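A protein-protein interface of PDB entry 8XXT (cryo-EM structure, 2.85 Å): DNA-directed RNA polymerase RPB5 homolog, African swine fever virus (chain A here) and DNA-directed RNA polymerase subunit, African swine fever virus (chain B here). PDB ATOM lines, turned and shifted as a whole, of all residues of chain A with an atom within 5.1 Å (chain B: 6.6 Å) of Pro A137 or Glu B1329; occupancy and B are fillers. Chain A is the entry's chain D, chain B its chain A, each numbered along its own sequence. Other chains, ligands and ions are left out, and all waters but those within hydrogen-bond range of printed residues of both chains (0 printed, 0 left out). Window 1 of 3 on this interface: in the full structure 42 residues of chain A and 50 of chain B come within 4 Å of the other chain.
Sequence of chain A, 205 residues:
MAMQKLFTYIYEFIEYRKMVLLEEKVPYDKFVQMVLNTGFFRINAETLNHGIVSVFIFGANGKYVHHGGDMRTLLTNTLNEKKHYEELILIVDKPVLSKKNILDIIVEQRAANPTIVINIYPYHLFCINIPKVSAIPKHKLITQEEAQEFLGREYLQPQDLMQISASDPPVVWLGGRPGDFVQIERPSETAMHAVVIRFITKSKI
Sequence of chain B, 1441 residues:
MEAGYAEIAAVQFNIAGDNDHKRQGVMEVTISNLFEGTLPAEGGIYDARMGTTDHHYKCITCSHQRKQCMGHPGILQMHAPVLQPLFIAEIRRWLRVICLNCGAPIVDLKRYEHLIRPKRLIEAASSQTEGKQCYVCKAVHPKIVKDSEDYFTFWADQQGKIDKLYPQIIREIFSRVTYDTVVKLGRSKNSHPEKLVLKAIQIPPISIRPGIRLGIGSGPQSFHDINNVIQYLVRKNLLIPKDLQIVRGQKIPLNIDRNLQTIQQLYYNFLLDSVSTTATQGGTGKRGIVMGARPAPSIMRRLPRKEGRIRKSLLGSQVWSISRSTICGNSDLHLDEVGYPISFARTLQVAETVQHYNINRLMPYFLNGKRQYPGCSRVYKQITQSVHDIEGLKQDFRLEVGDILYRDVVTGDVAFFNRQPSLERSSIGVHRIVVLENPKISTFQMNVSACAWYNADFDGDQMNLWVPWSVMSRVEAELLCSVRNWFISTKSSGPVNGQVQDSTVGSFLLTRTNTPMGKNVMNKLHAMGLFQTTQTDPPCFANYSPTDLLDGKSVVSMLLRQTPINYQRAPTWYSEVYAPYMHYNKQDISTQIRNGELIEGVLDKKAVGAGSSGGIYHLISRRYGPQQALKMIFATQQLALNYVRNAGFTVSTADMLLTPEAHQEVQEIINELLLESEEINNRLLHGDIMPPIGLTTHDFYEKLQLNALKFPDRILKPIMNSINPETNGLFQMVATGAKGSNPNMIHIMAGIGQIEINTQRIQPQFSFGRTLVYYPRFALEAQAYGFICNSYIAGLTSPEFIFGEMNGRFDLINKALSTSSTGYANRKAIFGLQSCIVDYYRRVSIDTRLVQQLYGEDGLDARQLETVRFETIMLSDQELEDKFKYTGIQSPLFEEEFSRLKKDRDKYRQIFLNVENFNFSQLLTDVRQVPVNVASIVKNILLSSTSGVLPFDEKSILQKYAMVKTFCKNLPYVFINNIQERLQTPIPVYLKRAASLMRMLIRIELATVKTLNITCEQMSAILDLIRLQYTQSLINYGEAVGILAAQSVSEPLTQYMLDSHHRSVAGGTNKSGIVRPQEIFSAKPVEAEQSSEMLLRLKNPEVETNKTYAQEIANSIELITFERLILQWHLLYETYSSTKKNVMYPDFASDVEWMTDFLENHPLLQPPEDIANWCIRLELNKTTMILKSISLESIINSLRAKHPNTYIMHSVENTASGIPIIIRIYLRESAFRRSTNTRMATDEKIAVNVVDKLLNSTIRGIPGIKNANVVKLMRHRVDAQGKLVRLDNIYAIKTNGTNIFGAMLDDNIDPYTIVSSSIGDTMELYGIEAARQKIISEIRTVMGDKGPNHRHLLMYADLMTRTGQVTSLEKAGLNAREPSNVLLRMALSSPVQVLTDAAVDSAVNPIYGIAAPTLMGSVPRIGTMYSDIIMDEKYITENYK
A ring nitrogen (ND1) of His A139 sits at hydrogen-bond distance from the backbone carbonyl oxygen of Pro A137 (2.8 Å). The backbone NH of Ile A184 lies within hydrogen-bond range of the backbone carbonyl oxygen of Val A196. SD of Met B1323 sits close to N of Ile B1328 (3.7 Å).
Pro A137 touches just one residue of chain B: Glu B1329. Glu B1329 touches five residues of chain A. Printed residues of chain A within 4 Å of Gln B1333: Pro A187. Of the printed residues of chain A, Gly B1327 touches Asp A168. Printed residues of chain A within 4 Å of Arg B1332: Arg A186. Printed residues of chain B within 4 Å of Arg A186: Glu B1329 and Arg B1332. The nearest residue of chain B that does not touch Pro A137 is Ala B1330 (4.4 Å). The nearest residue of chain A that does not touch Glu B1329 is Val A196 (4.6 Å).
Among the printed residues, merely in contact across the chains: Asp A168 with Gly B1327, Ile A184 with Glu B1329, Ile A136 with Tyr B1326, His A139 with Glu B1329, Ala A135 with Ala B1330, Pro A137 with Glu B1329 and Asp A168 with Met B1323.
N of Ile B1328 lies within hydrogen-bond range of OD1 of Asp A168 (3.2 Å). The guanidinium group of Arg A186 lies close to the guanidinium group of Arg B1332 (3.2 Å). The side-chain carboxylate (OE1) of Glu B1329 lies within salt-bridge range of the guanidinium group (NH2) of Arg A186, at 3.1 Å. The side-chain amide nitrogen of Gln B1333 is in hydrogen-bond range of the backbone carbonyl oxygen of Pro A187 (2.9 Å). The backbone carbonyl oxygen (O) of Ser A134 lies within hydrogen-bond range of the side-chain amide nitrogen (ND2) of Asn B914. The guanidinium group of Arg A198 is in salt-bridge range of the side-chain carboxylate of Glu B1329 (2.9 Å). O of Thr B1361 is in hydrogen-bond range of NH2 of Arg A198 (2.4 Å).
Printed residues of chain B that touch a printed residue of chain A: Asn B914, Met B1323, Tyr B1326, Gly B1327, Ile B1328, Glu B1329, Ala B1330, Arg B1332, Gln B1333 and Thr B1361. Hydrophobic or aromatic side chains of chain B within 4 Å of the printed part of chain A: Met B1323, Tyr B1326, Ile B1328 and Ala B1330. Hydrophobic or aromatic side chains of chain A within 4 Å of the printed part of chain B: Ile A136, Pro A137, His A139 and Ile A184. Among the printed residues, 14 pairs touch across the chains. Among the printed residues, Asp or Glu carboxylates within 4 Å of a Lys or Arg side-chain nitrogen of the other chain: Arg A186 with Glu B1329 and Arg A198 with Glu B1329.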
ATOM      1  N   SER A 134     -11.638  20.119 -26.179  1.00  0.00           N
ATOM      2  CA  SER A 134     -10.182  20.054 -26.172  1.00  0.00           C
ATOM      3  C   SER A 134      -9.573  21.258 -25.464  1.00  0.00           C
ATOM      4  O   SER A 134      -8.604  21.117 -24.711  1.00  0.00           O
ATOM      5  CB  SER A 134      -9.655  19.961 -27.602  1.00  0.00           C
ATOM      6  OG  SER A 134      -9.901  21.164 -28.307  1.00  0.00           O
ATOM      7  N   ALA A 135     -10.128  22.449 -25.695  1.00  0.00           N
ATOM      8  CA  ALA A 135      -9.550  23.667 -25.143  1.00  0.00           C
ATOM      9  C   ALA A 135      -9.691  23.753 -23.630  1.00  0.00           C
ATOM     10  O   ALA A 135      -8.908  24.460 -22.989  1.00  0.00           O
ATOM     11  CB  ALA A 135     -10.190  24.890 -25.792  1.00  0.00           C
ATOM     12  N   ILE A 136     -10.658  23.057 -23.050  1.00  0.00           N
ATOM     13  CA  ILE A 136     -10.886  23.082 -21.609  1.00  0.00           C
ATOM     14  C   ILE A 136     -10.049  21.973 -20.980  1.00  0.00           C
ATOM     15  O   ILE A 136     -10.302  20.792 -21.263  1.00  0.00           O
ATOM     16  CB  ILE A 136     -12.370  22.895 -21.278  1.00  0.00           C
ATOM     17  CG1 ILE A 136     -13.179  24.104 -21.744  1.00  0.00           C
ATOM     18  CG2 ILE A 136     -12.558  22.662 -19.795  1.00  0.00           C
ATOM     19  CD1 ILE A 136     -14.664  23.945 -21.550  1.00  0.00           C
ATOM     20  N   PRO A 137      -9.070  22.294 -20.131  1.00  0.00           N
ATOM     21  CA  PRO A 137      -8.310  21.237 -19.454  1.00  0.00           C
ATOM     22  C   PRO A 137      -9.165  20.490 -18.448  1.00  0.00           C
ATOM     23  O   PRO A 137     -10.334  20.831 -18.249  1.00  0.00           O
ATOM     24  CB  PRO A 137      -7.169  22.000 -18.775  1.00  0.00           C
ATOM     25  CG  PRO A 137      -7.669  23.380 -18.633  1.00  0.00           C
ATOM     26  CD  PRO A 137      -8.565  23.635 -19.802  1.00  0.00           C
ATOM     27  N   LYS A 138      -8.605  19.471 -17.809  1.00  0.00           N
ATOM     28  CA  LYS A 138      -9.387  18.629 -16.915  1.00  0.00           C
ATOM     29  C   LYS A 138      -9.540  19.310 -15.561  1.00  0.00           C
ATOM     30  O   LYS A 138      -8.548  19.675 -14.925  1.00  0.00           O
ATOM     31  CB  LYS A 138      -8.730  17.260 -16.763  1.00  0.00           C
ATOM     32  CG  LYS A 138      -9.684  16.106 -16.988  1.00  0.00           C
ATOM     33  CD  LYS A 138     -10.174  16.092 -18.428  1.00  0.00           C
ATOM     34  CE  LYS A 138     -11.180  14.981 -18.667  1.00  0.00           C
ATOM     35  NZ  LYS A 138     -11.746  15.043 -20.042  1.00  0.00           N
ATOM     36  N   HIS A 139     -10.785  19.475 -15.125  1.00  0.00           N
ATOM     37  CA  HIS A 139     -11.115  20.038 -13.825  1.00  0.00           C
ATOM     38  C   HIS A 139     -11.720  18.953 -12.947  1.00  0.00           C
ATOM     39  O   HIS A 139     -12.460  18.093 -13.432  1.00  0.00           O
ATOM     40  CB  HIS A 139     -12.109  21.194 -13.956  1.00  0.00           C
ATOM     41  CG  HIS A 139     -11.578  22.384 -14.692  1.00  0.00           C
ATOM     42  ND1 HIS A 139     -11.033  22.297 -15.953  1.00  0.00           N
ATOM     43  CD2 HIS A 139     -11.538  23.693 -14.354  1.00  0.00           C
ATOM     44  CE1 HIS A 139     -10.663  23.500 -16.354  1.00  0.00           C
ATOM     45  NE2 HIS A 139     -10.960  24.365 -15.402  1.00  0.00           N
ATOM     46  N   ASP A 168     -18.072  29.347 -13.981  1.00  0.00           N
ATOM     47  CA  ASP A 168     -17.214  28.806 -15.026  1.00  0.00           C
ATOM     48  C   ASP A 168     -17.806  27.501 -15.542  1.00  0.00           C
ATOM     49  O   ASP A 168     -18.230  26.663 -14.738  1.00  0.00           O
ATOM     50  CB  ASP A 168     -15.805  28.582 -14.485  1.00  0.00           C
ATOM     51  CG  ASP A 168     -14.731  28.958 -15.480  1.00  0.00           C
ATOM     52  OD1 ASP A 168     -14.770  30.092 -15.993  1.00  0.00           O
ATOM     53  OD2 ASP A 168     -13.845  28.120 -15.742  1.00  0.00           O
ATOM     54  N   ILE A 184      -6.844  21.419 -11.331  1.00  0.00           N
ATOM     55  CA  ILE A 184      -6.826  21.527 -12.783  1.00  0.00           C
ATOM     56  C   ILE A 184      -5.535  20.921 -13.308  1.00  0.00           C
ATOM     57  O   ILE A 184      -4.447  21.248 -12.822  1.00  0.00           O
ATOM     58  CB  ILE A 184      -6.968  22.990 -13.233  1.00  0.00           C
ATOM     59  CG1 ILE A 184      -8.156  23.629 -12.519  1.00  0.00           C
ATOM     60  CG2 ILE A 184      -7.121  23.075 -14.738  1.00  0.00           C
ATOM     61  CD1 ILE A 184      -8.439  25.024 -12.946  1.00  0.00           C
ATOM     62  N   GLU A 185      -5.659  20.039 -14.297  1.00  0.00           N
ATOM     63  CA  GLU A 185      -4.517  19.409 -14.958  1.00  0.00           C
ATOM     64  C   GLU A 185      -4.324  20.099 -16.303  1.00  0.00           C
ATOM     65  O   GLU A 185      -4.766  19.609 -17.339  1.00  0.00           O
ATOM     66  CB  GLU A 185      -4.744  17.912 -15.123  1.00  0.00           C
ATOM     67  CG  GLU A 185      -4.216  17.075 -13.978  1.00  0.00           C
ATOM     68  CD  GLU A 185      -2.877  16.445 -14.292  1.00  0.00           C
ATOM     69  OE1 GLU A 185      -2.382  16.631 -15.423  1.00  0.00           O
ATOM     70  OE2 GLU A 185      -2.319  15.762 -13.408  1.00  0.00           O
ATOM     71  N   ARG A 186      -3.654  21.239 -16.281  1.00  0.00           N
ATOM     72  CA  ARG A 186      -3.482  22.017 -17.499  1.00  0.00           C
ATOM     73  C   ARG A 186      -2.344  21.455 -18.333  1.00  0.00           C
ATOM     74  O   ARG A 186      -1.267  21.182 -17.790  1.00  0.00           O
ATOM     75  CB  ARG A 186      -3.210  23.485 -17.175  1.00  0.00           C
ATOM     76  CG  ARG A 186      -2.023  23.706 -16.270  1.00  0.00           C
ATOM     77  CD  ARG A 186      -1.959  25.111 -15.699  1.00  0.00           C
ATOM     78  NE  ARG A 186      -3.188  25.568 -15.066  1.00  0.00           N
ATOM     79  CZ  ARG A 186      -3.353  26.791 -14.579  1.00  0.00           C
ATOM     80  NH1 ARG A 186      -2.378  27.683 -14.606  1.00  0.00           N
ATOM     81  NH2 ARG A 186      -4.524  27.126 -14.049  1.00  0.00           N
ATOM     82  N   PRO A 187      -2.544  21.229 -19.630  1.00  0.00           N
ATOM     83  CA  PRO A 187      -1.411  20.892 -20.497  1.00  0.00           C
ATOM     84  C   PRO A 187      -0.424  22.045 -20.560  1.00  0.00           C
ATOM     85  O   PRO A 187      -0.811  23.213 -20.601  1.00  0.00           O
ATOM     86  CB  PRO A 187      -2.069  20.638 -21.857  1.00  0.00           C
ATOM     87  CG  PRO A 187      -3.345  21.395 -21.801  1.00  0.00           C
ATOM     88  CD  PRO A 187      -3.805  21.320 -20.381  1.00  0.00           C
ATOM     89  N   VAL A 196      -2.612  22.717 -10.800  1.00  0.00           N
ATOM     90  CA  VAL A 196      -2.875  23.841  -9.916  1.00  0.00           C
ATOM     91  C   VAL A 196      -4.187  23.578  -9.191  1.00  0.00           C
ATOM     92  O   VAL A 196      -4.998  22.749  -9.604  1.00  0.00           O
ATOM     93  CB  VAL A 196      -2.944  25.189 -10.662  1.00  0.00           C
ATOM     94  CG1 VAL A 196      -1.781  25.332 -11.619  1.00  0.00           C
ATOM     95  CG2 VAL A 196      -4.261  25.320 -11.388  1.00  0.00           C
ATOM     96  N   ARG A 198      -7.422  25.829  -7.611  1.00  0.00           N
ATOM     97  CA  ARG A 198      -8.059  27.136  -7.621  1.00  0.00           C
ATOM     98  C   ARG A 198      -9.202  27.167  -6.618  1.00  0.00           C
ATOM     99  O   ARG A 198      -9.775  26.133  -6.268  1.00  0.00           O
ATOM    100  CB  ARG A 198      -8.574  27.494  -9.015  1.00  0.00           C
ATOM    101  CG  ARG A 198      -7.481  27.587 -10.056  1.00  0.00           C
ATOM    102  CD  ARG A 198      -7.998  28.130 -11.370  1.00  0.00           C
ATOM    103  NE  ARG A 198      -8.017  29.584 -11.401  1.00  0.00           N
ATOM    104  CZ  ARG A 198      -7.392  30.319 -12.309  1.00  0.00           C
ATOM    105  NH1 ARG A 198      -6.661  29.767 -13.260  1.00  0.00           N
ATOM    106  NH2 ARG A 198      -7.500  31.641 -12.257  1.00  0.00           N
ATOM    107  N   ASN B 914      -3.388  17.400 -27.934  1.00  0.00           N
ATOM    108  CA  ASN B 914      -4.398  18.302 -27.397  1.00  0.00           C
ATOM    109  C   ASN B 914      -3.995  19.754 -27.594  1.00  0.00           C
ATOM    110  O   ASN B 914      -4.825  20.592 -27.957  1.00  0.00           O
ATOM    111  CB  ASN B 914      -4.626  18.008 -25.916  1.00  0.00           C
ATOM    112  CG  ASN B 914      -5.963  18.496 -25.426  1.00  0.00           C
ATOM    113  OD1 ASN B 914      -7.008  18.091 -25.932  1.00  0.00           O
ATOM    114  ND2 ASN B 914      -5.944  19.373 -24.432  1.00  0.00           N
ATOM    115  N   MET B1323     -13.277  33.115 -23.080  1.00  0.00           N
ATOM    116  CA  MET B1323     -13.554  33.188 -21.651  1.00  0.00           C
ATOM    117  C   MET B1323     -15.024  32.926 -21.354  1.00  0.00           C
ATOM    118  O   MET B1323     -15.352  32.160 -20.442  1.00  0.00           O
ATOM    119  CB  MET B1323     -13.134  34.554 -21.113  1.00  0.00           C
ATOM    120  CG  MET B1323     -13.567  34.823 -19.690  1.00  0.00           C
ATOM    121  SD  MET B1323     -12.686  33.809 -18.503  1.00  0.00           S
ATOM    122  CE  MET B1323     -13.982  33.474 -17.318  1.00  0.00           C
ATOM    123  N   TYR B1326     -15.834  29.019 -22.857  1.00  0.00           N
ATOM    124  CA  TYR B1326     -15.081  27.877 -22.353  1.00  0.00           C
ATOM    125  C   TYR B1326     -14.713  27.994 -20.881  1.00  0.00           C
ATOM    126  O   TYR B1326     -14.943  27.052 -20.120  1.00  0.00           O
ATOM    127  CB  TYR B1326     -13.811  27.685 -23.183  1.00  0.00           C
ATOM    128  CG  TYR B1326     -14.073  27.223 -24.597  1.00  0.00           C
ATOM    129  CD1 TYR B1326     -15.169  26.427 -24.894  1.00  0.00           C
ATOM    130  CD2 TYR B1326     -13.228  27.587 -25.635  1.00  0.00           C
ATOM    131  CE1 TYR B1326     -15.411  26.003 -26.180  1.00  0.00           C
ATOM    132  CE2 TYR B1326     -13.465  27.169 -26.926  1.00  0.00           C
ATOM    133  CZ  TYR B1326     -14.558  26.377 -27.192  1.00  0.00           C
ATOM    134  OH  TYR B1326     -14.799  25.956 -28.476  1.00  0.00           O
ATOM    135  N   GLY B1327     -14.145  29.115 -20.458  1.00  0.00           N
ATOM    136  CA  GLY B1327     -13.798  29.323 -19.071  1.00  0.00           C
ATOM    137  C   GLY B1327     -12.486  30.057 -18.924  1.00  0.00           C
ATOM    138  O   GLY B1327     -11.847  30.455 -19.895  1.00  0.00           O
ATOM    139  N   ILE B1328     -12.085  30.232 -17.664  1.00  0.00           N
ATOM    140  CA  ILE B1328     -10.861  30.968 -17.374  1.00  0.00           C
ATOM    141  C   ILE B1328      -9.636  30.186 -17.819  1.00  0.00           C
ATOM    142  O   ILE B1328      -8.604  30.777 -18.159  1.00  0.00           O
ATOM    143  CB  ILE B1328     -10.794  31.329 -15.878  1.00  0.00           C
ATOM    144  CG1 ILE B1328      -9.678  32.338 -15.629  1.00  0.00           C
ATOM    145  CG2 ILE B1328     -10.580  30.095 -15.029  1.00  0.00           C
ATOM    146  CD1 ILE B1328      -9.837  33.606 -16.415  1.00  0.00           C
ATOM    147  N   GLU B1329      -9.716  28.856 -17.827  1.00  0.00           N
ATOM    148  CA  GLU B1329      -8.540  28.062 -18.157  1.00  0.00           C
ATOM    149  C   GLU B1329      -8.263  28.051 -19.654  1.00  0.00           C
ATOM    150  O   GLU B1329      -7.103  28.119 -20.070  1.00  0.00           O
ATOM    151  CB  GLU B1329      -8.709  26.643 -17.633  1.00  0.00           C
ATOM    152  CG  GLU B1329      -8.395  26.524 -16.162  1.00  0.00           C
ATOM    153  CD  GLU B1329      -6.964  26.893 -15.840  1.00  0.00           C
ATOM    154  OE1 GLU B1329      -6.095  26.784 -16.730  1.00  0.00           O
ATOM    155  OE2 GLU B1329      -6.706  27.300 -14.690  1.00  0.00           O
ATOM    156  N   ALA B1330      -9.307  27.957 -20.477  1.00  0.00           N
ATOM    157  CA  ALA B1330      -9.106  28.091 -21.912  1.00  0.00           C
ATOM    158  C   ALA B1330      -8.777  29.526 -22.288  1.00  0.00           C
ATOM    159  O   ALA B1330      -8.047  29.760 -23.256  1.00  0.00           O
ATOM    160  CB  ALA B1330     -10.339  27.611 -22.667  1.00  0.00           C
ATOM    161  N   ALA B1331      -9.310  30.495 -21.542  1.00  0.00           N
ATOM    162  CA  ALA B1331      -8.906  31.881 -21.740  1.00  0.00           C
ATOM    163  C   ALA B1331      -7.437  32.069 -21.398  1.00  0.00           C
ATOM    164  O   ALA B1331      -6.718  32.801 -22.088  1.00  0.00           O
ATOM    165  CB  ALA B1331      -9.777  32.811 -20.900  1.00  0.00           C
ATOM    166  N   ARG B1332      -6.971  31.417 -20.331  1.00  0.00           N
ATOM    167  CA  ARG B1332      -5.556  31.482 -19.988  1.00  0.00           C
ATOM    168  C   ARG B1332      -4.699  30.872 -21.085  1.00  0.00           C
ATOM    169  O   ARG B1332      -3.654  31.425 -21.445  1.00  0.00           O
ATOM    170  CB  ARG B1332      -5.299  30.774 -18.662  1.00  0.00           C
ATOM    171  CG  ARG B1332      -3.841  30.773 -18.263  1.00  0.00           C
ATOM    172  CD  ARG B1332      -3.503  29.592 -17.385  1.00  0.00           C
ATOM    173  NE  ARG B1332      -2.062  29.458 -17.219  1.00  0.00           N
ATOM    174  CZ  ARG B1332      -1.336  28.488 -17.753  1.00  0.00           C
ATOM    175  NH1 ARG B1332      -1.887  27.531 -18.479  1.00  0.00           N
ATOM    176  NH2 ARG B1332      -0.022  28.477 -17.552  1.00  0.00           N
ATOM    177  N   GLN B1333      -5.120  29.728 -21.628  1.00  0.00           N
ATOM    178  CA  GLN B1333      -4.395  29.138 -22.748  1.00  0.00           C
ATOM    179  C   GLN B1333      -4.507  29.991 -24.000  1.00  0.00           C
ATOM    180  O   GLN B1333      -3.570  30.035 -24.803  1.00  0.00           O
ATOM    181  CB  GLN B1333      -4.903  27.726 -23.028  1.00  0.00           C
ATOM    182  CG  GLN B1333      -4.484  26.700 -21.999  1.00  0.00           C
ATOM    183  CD  GLN B1333      -3.043  26.272 -22.158  1.00  0.00           C
ATOM    184  OE1 GLN B1333      -2.338  26.737 -23.052  1.00  0.00           O
ATOM    185  NE2 GLN B1333      -2.596  25.374 -21.292  1.00  0.00           N
ATOM    186  N   LYS B1334      -5.641  30.667 -24.190  1.00  0.00           N
ATOM    187  CA  LYS B1334      -5.790  31.535 -25.351  1.00  0.00           C
ATOM    188  C   LYS B1334      -4.833  32.714 -25.285  1.00  0.00           C
ATOM    189  O   LYS B1334      -4.295  33.143 -26.311  1.00  0.00           O
ATOM    190  CB  LYS B1334      -7.233  32.020 -25.465  1.00  0.00           C
ATOM    191  CG  LYS B1334      -7.563  32.645 -26.807  1.00  0.00           C
ATOM    192  CD  LYS B1334      -7.275  31.691 -27.952  1.00  0.00           C
ATOM    193  CE  LYS B1334      -8.076  30.406 -27.822  1.00  0.00           C
ATOM    194  NZ  LYS B1334      -7.621  29.372 -28.785  1.00  0.00           N
ATOM    195  N   THR B1361      -5.269  36.078 -15.559  1.00  0.00           N
ATOM    196  CA  THR B1361      -6.350  35.158 -15.239  1.00  0.00           C
ATOM    197  C   THR B1361      -6.315  34.681 -13.793  1.00  0.00           C
ATOM    198  O   THR B1361      -6.976  33.694 -13.462  1.00  0.00           O
ATOM    199  CB  THR B1361      -6.306  33.961 -16.182  1.00  0.00           C
ATOM    200  OG1 THR B1361      -5.081  33.249 -15.986  1.00  0.00           O
ATOM    201  CG2 THR B1361      -6.381  34.427 -17.620  1.00  0.00           C
